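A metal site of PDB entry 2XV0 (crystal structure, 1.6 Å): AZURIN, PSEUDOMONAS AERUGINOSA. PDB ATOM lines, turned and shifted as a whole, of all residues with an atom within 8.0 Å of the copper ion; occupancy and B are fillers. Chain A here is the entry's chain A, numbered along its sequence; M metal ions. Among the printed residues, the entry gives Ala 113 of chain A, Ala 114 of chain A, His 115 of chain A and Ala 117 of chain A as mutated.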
ATOM      1  N   GLY A   9       4.096  11.177   8.859  1.00  0.00           N
ATOM      2  CA  GLY A   9       5.428  11.736   8.535  1.00  0.00           C
ATOM      3  C   GLY A   9       5.928  11.019   7.287  1.00  0.00           C
ATOM      4  O   GLY A   9       5.997   9.806   7.271  1.00  0.00           O
ATOM      5  N   ASN A  10       6.254  11.768   6.257  1.00  0.00           N
ATOM      6  CA  ASN A  10       6.509  11.162   4.925  1.00  0.00           C
ATOM      7  C   ASN A  10       7.971  11.186   4.487  1.00  0.00           C
ATOM      8  O   ASN A  10       8.871  11.547   5.227  1.00  0.00           O
ATOM      9  CB  ASN A  10       5.603  11.772   3.850  1.00  0.00           C
ATOM     10  CG  ASN A  10       5.975  13.200   3.522  1.00  0.00           C
ATOM     11  OD1 ASN A  10       7.008  13.692   3.980  1.00  0.00           O
ATOM     12  ND2 ASN A  10       5.130  13.896   2.740  1.00  0.00           N
ATOM     13  N   MET A  13      10.121  14.567   4.561  1.00  0.00           N
ATOM     14  CA  MET A  13      10.485  15.228   5.843  1.00  0.00           C
ATOM     15  C   MET A  13       9.418  16.237   6.258  1.00  0.00           C
ATOM     16  O   MET A  13       9.700  17.359   6.700  1.00  0.00           O
ATOM     17  CB  MET A  13      11.901  15.848   5.766  1.00  0.00           C
ATOM     18  CG  MET A  13      12.507  16.080   7.127  1.00  0.00           C
ATOM     19  SD  MET A  13      14.107  16.944   7.108  1.00  0.00           S
ATOM     20  CE  MET A  13      13.603  18.639   6.767  1.00  0.00           C
ATOM     21  N   GLN A  14       8.161  15.826   6.085  1.00  0.00           N
ATOM     22  CA  GLN A  14       7.046  16.611   6.561  1.00  0.00           C
ATOM     23  C   GLN A  14       5.949  15.810   7.295  1.00  0.00           C
ATOM     24  O   GLN A  14       5.593  14.719   6.882  1.00  0.00           O
ATOM     25  CB  GLN A  14       6.433  17.368   5.413  1.00  0.00           C
ATOM     26  CG  GLN A  14       5.744  16.543   4.477  1.00  0.00           C
ATOM     27  N   PHE A  15       5.394  16.413   8.347  1.00  0.00           N
ATOM     28  CA  PHE A  15       4.146  15.926   8.931  1.00  0.00           C
ATOM     29  C   PHE A  15       3.007  16.505   8.064  1.00  0.00           C
ATOM     30  O   PHE A  15       3.174  17.576   7.442  1.00  0.00           O
ATOM     31  CB  PHE A  15       3.939  16.447  10.339  1.00  0.00           C
ATOM     32  CG  PHE A  15       4.821  15.846  11.386  1.00  0.00           C
ATOM     33  CD1 PHE A  15       4.825  14.467  11.603  1.00  0.00           C
ATOM     34  CD2 PHE A  15       5.553  16.661  12.228  1.00  0.00           C
ATOM     35  CE1 PHE A  15       5.601  13.916  12.611  1.00  0.00           C
ATOM     36  CE2 PHE A  15       6.327  16.121  13.259  1.00  0.00           C
ATOM     37  CZ  PHE A  15       6.312  14.720  13.463  1.00  0.00           C
ATOM     38  N   LEU A  33       0.693   7.778  14.866  1.00  0.00           N
ATOM     39  CA  LEU A  33       1.681   8.196  13.850  1.00  0.00           C
ATOM     40  C   LEU A  33       1.888   7.089  12.802  1.00  0.00           C
ATOM     41  O   LEU A  33       2.062   5.917  13.172  1.00  0.00           O
ATOM     42  CB  LEU A  33       3.014   8.518  14.543  1.00  0.00           C
ATOM     43  CG  LEU A  33       4.167   9.019  13.683  1.00  0.00           C
ATOM     44  CD1 LEU A  33       3.886  10.416  13.067  1.00  0.00           C
ATOM     45  CD2 LEU A  33       5.517   9.001  14.448  1.00  0.00           C
ATOM     46  N   HIS A  35       3.888   6.403   8.628  1.00  0.00           N
ATOM     47  CA  HIS A  35       4.944   6.883   7.739  1.00  0.00           C
ATOM     48  C   HIS A  35       4.669   6.385   6.305  1.00  0.00           C
ATOM     49  O   HIS A  35       5.208   5.371   5.872  1.00  0.00           O
ATOM     50  CB  HIS A  35       6.278   6.371   8.222  1.00  0.00           C
ATOM     51  CG  HIS A  35       7.476   6.948   7.522  1.00  0.00           C
ATOM     52  ND1 HIS A  35       7.489   7.224   6.166  1.00  0.00           N
ATOM     53  CD2 HIS A  35       8.726   7.193   7.986  1.00  0.00           C
ATOM     54  CE1 HIS A  35       8.701   7.661   5.840  1.00  0.00           C
ATOM     55  NE2 HIS A  35       9.465   7.658   6.927  1.00  0.00           N
ATOM     56  N   MET A  44      15.102   7.803   6.682  1.00  0.00           N
ATOM     57  CA  MET A  44      14.119   8.862   6.980  1.00  0.00           C
ATOM     58  C   MET A  44      13.125   8.379   8.038  1.00  0.00           C
ATOM     59  O   MET A  44      11.936   8.309   7.758  1.00  0.00           O
ATOM     60  CB  MET A  44      13.396   9.276   5.677  1.00  0.00           C
ATOM     61  CG  MET A  44      12.548  10.570   5.759  1.00  0.00           C
ATOM     62  SD  MET A  44      13.421  12.056   6.327  1.00  0.00           S
ATOM     63  CE  MET A  44      14.536  12.364   4.945  1.00  0.00           C
ATOM     64  N   GLY A  45      13.626   8.063   9.224  1.00  0.00           N
ATOM     65  CA  GLY A  45      12.752   7.711  10.325  1.00  0.00           C
ATOM     66  C   GLY A  45      12.189   8.960  10.995  1.00  0.00           C
ATOM     67  O   GLY A  45      12.858   9.994  11.093  1.00  0.00           O
ATOM     68  N   HIS A  46      10.971   8.839  11.518  1.00  0.00           N
ATOM     69  CA  HIS A  46      10.316   9.928  12.220  1.00  0.00           C
ATOM     70  C   HIS A  46       9.764   9.451  13.562  1.00  0.00           C
ATOM     71  O   HIS A  46       9.323   8.302  13.700  1.00  0.00           O
ATOM     72  CB  HIS A  46       9.089  10.438  11.449  1.00  0.00           C
ATOM     73  CG  HIS A  46       9.372  10.938  10.072  1.00  0.00           C
ATOM     74  ND1 HIS A  46      10.271  11.944   9.821  1.00  0.00           N
ATOM     75  CD2 HIS A  46       8.841  10.602   8.885  1.00  0.00           C
ATOM     76  CE1 HIS A  46      10.305  12.185   8.519  1.00  0.00           C
ATOM     77  NE2 HIS A  46       9.435  11.388   7.929  1.00  0.00           N
ATOM     78  N   ASN A  47       9.760  10.357  14.531  1.00  0.00           N
ATOM     79  CA  ASN A  47       8.957  10.193  15.738  1.00  0.00           C
ATOM     80  C   ASN A  47       8.078  11.422  15.944  1.00  0.00           C
ATOM     81  O   ASN A  47       8.075  12.391  15.142  1.00  0.00           O
ATOM     82  CB  ASN A  47       9.771   9.780  16.966  1.00  0.00           C
ATOM     83  CG  ASN A  47      10.747  10.829  17.406  1.00  0.00           C
ATOM     84  OD1 ASN A  47      10.775  11.938  16.856  1.00  0.00           O
ATOM     85  ND2 ASN A  47      11.595  10.489  18.411  1.00  0.00           N
ATOM     86  N   TRP A  48       7.316  11.367  17.032  1.00  0.00           N
ATOM     87  CA  TRP A  48       6.450  12.476  17.422  1.00  0.00           C
ATOM     88  C   TRP A  48       6.697  12.696  18.909  1.00  0.00           C
ATOM     89  O   TRP A  48       6.583  11.754  19.720  1.00  0.00           O
ATOM     90  CB  TRP A  48       5.009  12.144  17.147  1.00  0.00           C
ATOM     91  CG  TRP A  48       4.018  13.200  17.404  1.00  0.00           C
ATOM     92  CD1 TRP A  48       3.477  14.053  16.499  1.00  0.00           C
ATOM     93  CD2 TRP A  48       3.374  13.479  18.666  1.00  0.00           C
ATOM     94  NE1 TRP A  48       2.559  14.897  17.127  1.00  0.00           N
ATOM     95  CE2 TRP A  48       2.475  14.552  18.456  1.00  0.00           C
ATOM     96  CE3 TRP A  48       3.478  12.940  19.960  1.00  0.00           C
ATOM     97  CZ2 TRP A  48       1.701  15.074  19.477  1.00  0.00           C
ATOM     98  CZ3 TRP A  48       2.669  13.452  20.970  1.00  0.00           C
ATOM     99  CH2 TRP A  48       1.801  14.504  20.725  1.00  0.00           C
ATOM    100  N   LEU A  86      10.615   5.758  17.008  1.00  0.00           N
ATOM    101  CA  LEU A  86      11.043   6.144  15.649  1.00  0.00           C
ATOM    102  C   LEU A  86      10.523   5.099  14.683  1.00  0.00           C
ATOM    103  O   LEU A  86      10.753   3.901  14.895  1.00  0.00           O
ATOM    104  CB  LEU A  86      12.562   6.173  15.554  1.00  0.00           C
ATOM    105  CG  LEU A  86      13.177   6.785  14.279  1.00  0.00           C
ATOM    106  CD1 LEU A  86      13.167   8.302  14.487  1.00  0.00           C
ATOM    107  CD2 LEU A  86      14.595   6.299  14.034  1.00  0.00           C
ATOM    108  N   ILE A  87       9.866   5.550  13.625  1.00  0.00           N
ATOM    109  CA  ILE A  87       9.306   4.644  12.620  1.00  0.00           C
ATOM    110  C   ILE A  87       9.806   4.951  11.216  1.00  0.00           C
ATOM    111  O   ILE A  87      10.097   6.124  10.885  1.00  0.00           O
ATOM    112  CB  ILE A  87       7.765   4.653  12.631  1.00  0.00           C
ATOM    113  CG1 ILE A  87       7.182   5.998  12.203  1.00  0.00           C
ATOM    114  CG2 ILE A  87       7.218   4.204  14.027  1.00  0.00           C
ATOM    115  CD1 ILE A  87       5.649   5.896  11.995  1.00  0.00           C
ATOM    116  N   PHE A 111       6.945  17.783  17.605  1.00  0.00           N
ATOM    117  CA  PHE A 111       8.048  17.771  16.673  1.00  0.00           C
ATOM    118  C   PHE A 111       8.623  16.367  16.517  1.00  0.00           C
ATOM    119  O   PHE A 111       8.409  15.487  17.361  1.00  0.00           O
ATOM    120  CB  PHE A 111       9.125  18.797  17.065  1.00  0.00           C
ATOM    121  CG  PHE A 111       9.672  18.601  18.448  1.00  0.00           C
ATOM    122  CD1 PHE A 111       9.051  19.175  19.539  1.00  0.00           C
ATOM    123  CD2 PHE A 111      10.851  17.909  18.659  1.00  0.00           C
ATOM    124  CE1 PHE A 111       9.565  18.992  20.804  1.00  0.00           C
ATOM    125  CE2 PHE A 111      11.358  17.718  19.924  1.00  0.00           C
ATOM    126  CZ  PHE A 111      10.712  18.263  21.002  1.00  0.00           C
ATOM    127  N   CYS A 112       9.369  16.217  15.440  1.00  0.00           N
ATOM    128  CA  CYS A 112      10.212  15.044  15.213  1.00  0.00           C
ATOM    129  C   CYS A 112      11.603  15.330  15.808  1.00  0.00           C
ATOM    130  O   CYS A 112      12.272  16.324  15.445  1.00  0.00           O
ATOM    131  CB  CYS A 112      10.349  14.768  13.701  1.00  0.00           C
ATOM    132  SG  CYS A 112      11.290  13.312  13.379  1.00  0.00           S
ATOM    133  N   ALA A 113      12.059  14.467  16.705  1.00  0.00           N
ATOM    134  CA  ALA A 113      13.389  14.673  17.301  1.00  0.00           C
ATOM    135  C   ALA A 113      14.512  14.437  16.296  1.00  0.00           C
ATOM    136  O   ALA A 113      15.540  15.070  16.432  1.00  0.00           O
ATOM    137  CB  ALA A 113      13.616  13.766  18.506  1.00  0.00           C
ATOM    138  N   ALA A 114      14.312  13.565  15.311  1.00  0.00           N
ATOM    139  CA  ALA A 114      15.317  13.340  14.222  1.00  0.00           C
ATOM    140  C   ALA A 114      15.423  14.544  13.287  1.00  0.00           C
ATOM    141  O   ALA A 114      16.493  14.881  12.792  1.00  0.00           O
ATOM    142  CB  ALA A 114      14.964  12.083  13.420  1.00  0.00           C
ATOM    143  N   HIS A 115      14.278  15.189  13.037  1.00  0.00           N
ATOM    144  CA  HIS A 115      14.161  16.289  12.078  1.00  0.00           C
ATOM    145  C   HIS A 115      13.348  17.378  12.746  1.00  0.00           C
ATOM    146  O   HIS A 115      12.172  17.539  12.479  1.00  0.00           O
ATOM    147  CB  HIS A 115      13.478  15.839  10.811  1.00  0.00           C
ATOM    148  CG  HIS A 115      14.051  14.586  10.221  1.00  0.00           C
ATOM    149  ND1 HIS A 115      13.354  13.400  10.204  1.00  0.00           N
ATOM    150  CD2 HIS A 115      15.258  14.341   9.635  1.00  0.00           C
ATOM    151  CE1 HIS A 115      14.099  12.469   9.632  1.00  0.00           C
ATOM    152  NE2 HIS A 115      15.247  13.012   9.263  1.00  0.00           N
ATOM    153  N   ALA A 116      14.027  18.157  13.596  1.00  0.00           N
ATOM    154  CA  ALA A 116      13.364  19.172  14.449  1.00  0.00           C
ATOM    155  C   ALA A 116      12.679  20.291  13.670  1.00  0.00           C
ATOM    156  O   ALA A 116      11.876  21.051  14.230  1.00  0.00           O
ATOM    157  CB  ALA A 116      14.387  19.751  15.476  1.00  0.00           C
ATOM    158  N   ALA A 117      13.000  20.407  12.387  1.00  0.00           N
ATOM    159  CA  ALA A 117      12.248  21.307  11.519  1.00  0.00           C
ATOM    160  C   ALA A 117      10.819  20.894  11.312  1.00  0.00           C
ATOM    161  O   ALA A 117      10.012  21.719  10.951  1.00  0.00           O
ATOM    162  CB  ALA A 117      12.959  21.484  10.147  1.00  0.00           C
ATOM    163  N   MET A 118      10.513  19.594  11.514  1.00  0.00           N
ATOM    164  CA  MET A 118       9.161  19.048  11.396  1.00  0.00           C
ATOM    165  C   MET A 118       8.479  19.311  12.739  1.00  0.00           C
ATOM    166  O   MET A 118       8.820  18.703  13.768  1.00  0.00           O
ATOM    167  CB  MET A 118       9.186  17.522  11.166  1.00  0.00           C
ATOM    168  CG  MET A 118       9.760  17.118   9.909  1.00  0.00           C
ATOM    169  SD  MET A 118       9.896  15.297   9.722  1.00  0.00           S
ATOM    170  CE  MET A 118       8.190  14.754  10.015  1.00  0.00           C
HETATM  171 CU    CU M   1      11.338  13.149  11.230  1.00  0.00          CU
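A ring nitrogen (ND1) of His 46 lies close to the side-chain sulfur of Met 118. A ring nitrogen (NE2) of His 46 lies within hydrogen-bond range of the backbone carbonyl oxygen (O) of Asn 10, at 2.8 Å. N of Ile 87 sits at hydrogen-bond distance from O of His 46, at 2.8 Å. The backbone carbonyl oxygen (O) of Met 118 lies within hydrogen-bond range of the backbone NH (N) of Cys 112, at 3.0 Å. The side-chain sulfur (SG) of Cys 112 lies close to the backbone NH (N) of Ala 114, at 3.6 Å. The side-chain sulfur (SG) of Cys 112 lies close to the backbone NH (N) of Asn 47. The side-chain sulfur (SD) of Met 44 lies close to a ring nitrogen (NE2) of His 115 (3.6 Å).
Gly 45 touches the copper ion.
The copper ion is bound by a ring nitrogen (ND1) of His 46 (2.1 Å), the side-chain sulfur of Cys 112 (2.2 Å) and a ring nitrogen (ND1) of His 115 (2.3 Å). Slightly farther from the copper ion lies the side-chain sulfur (SD) of Met 118 (3.0 Å).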
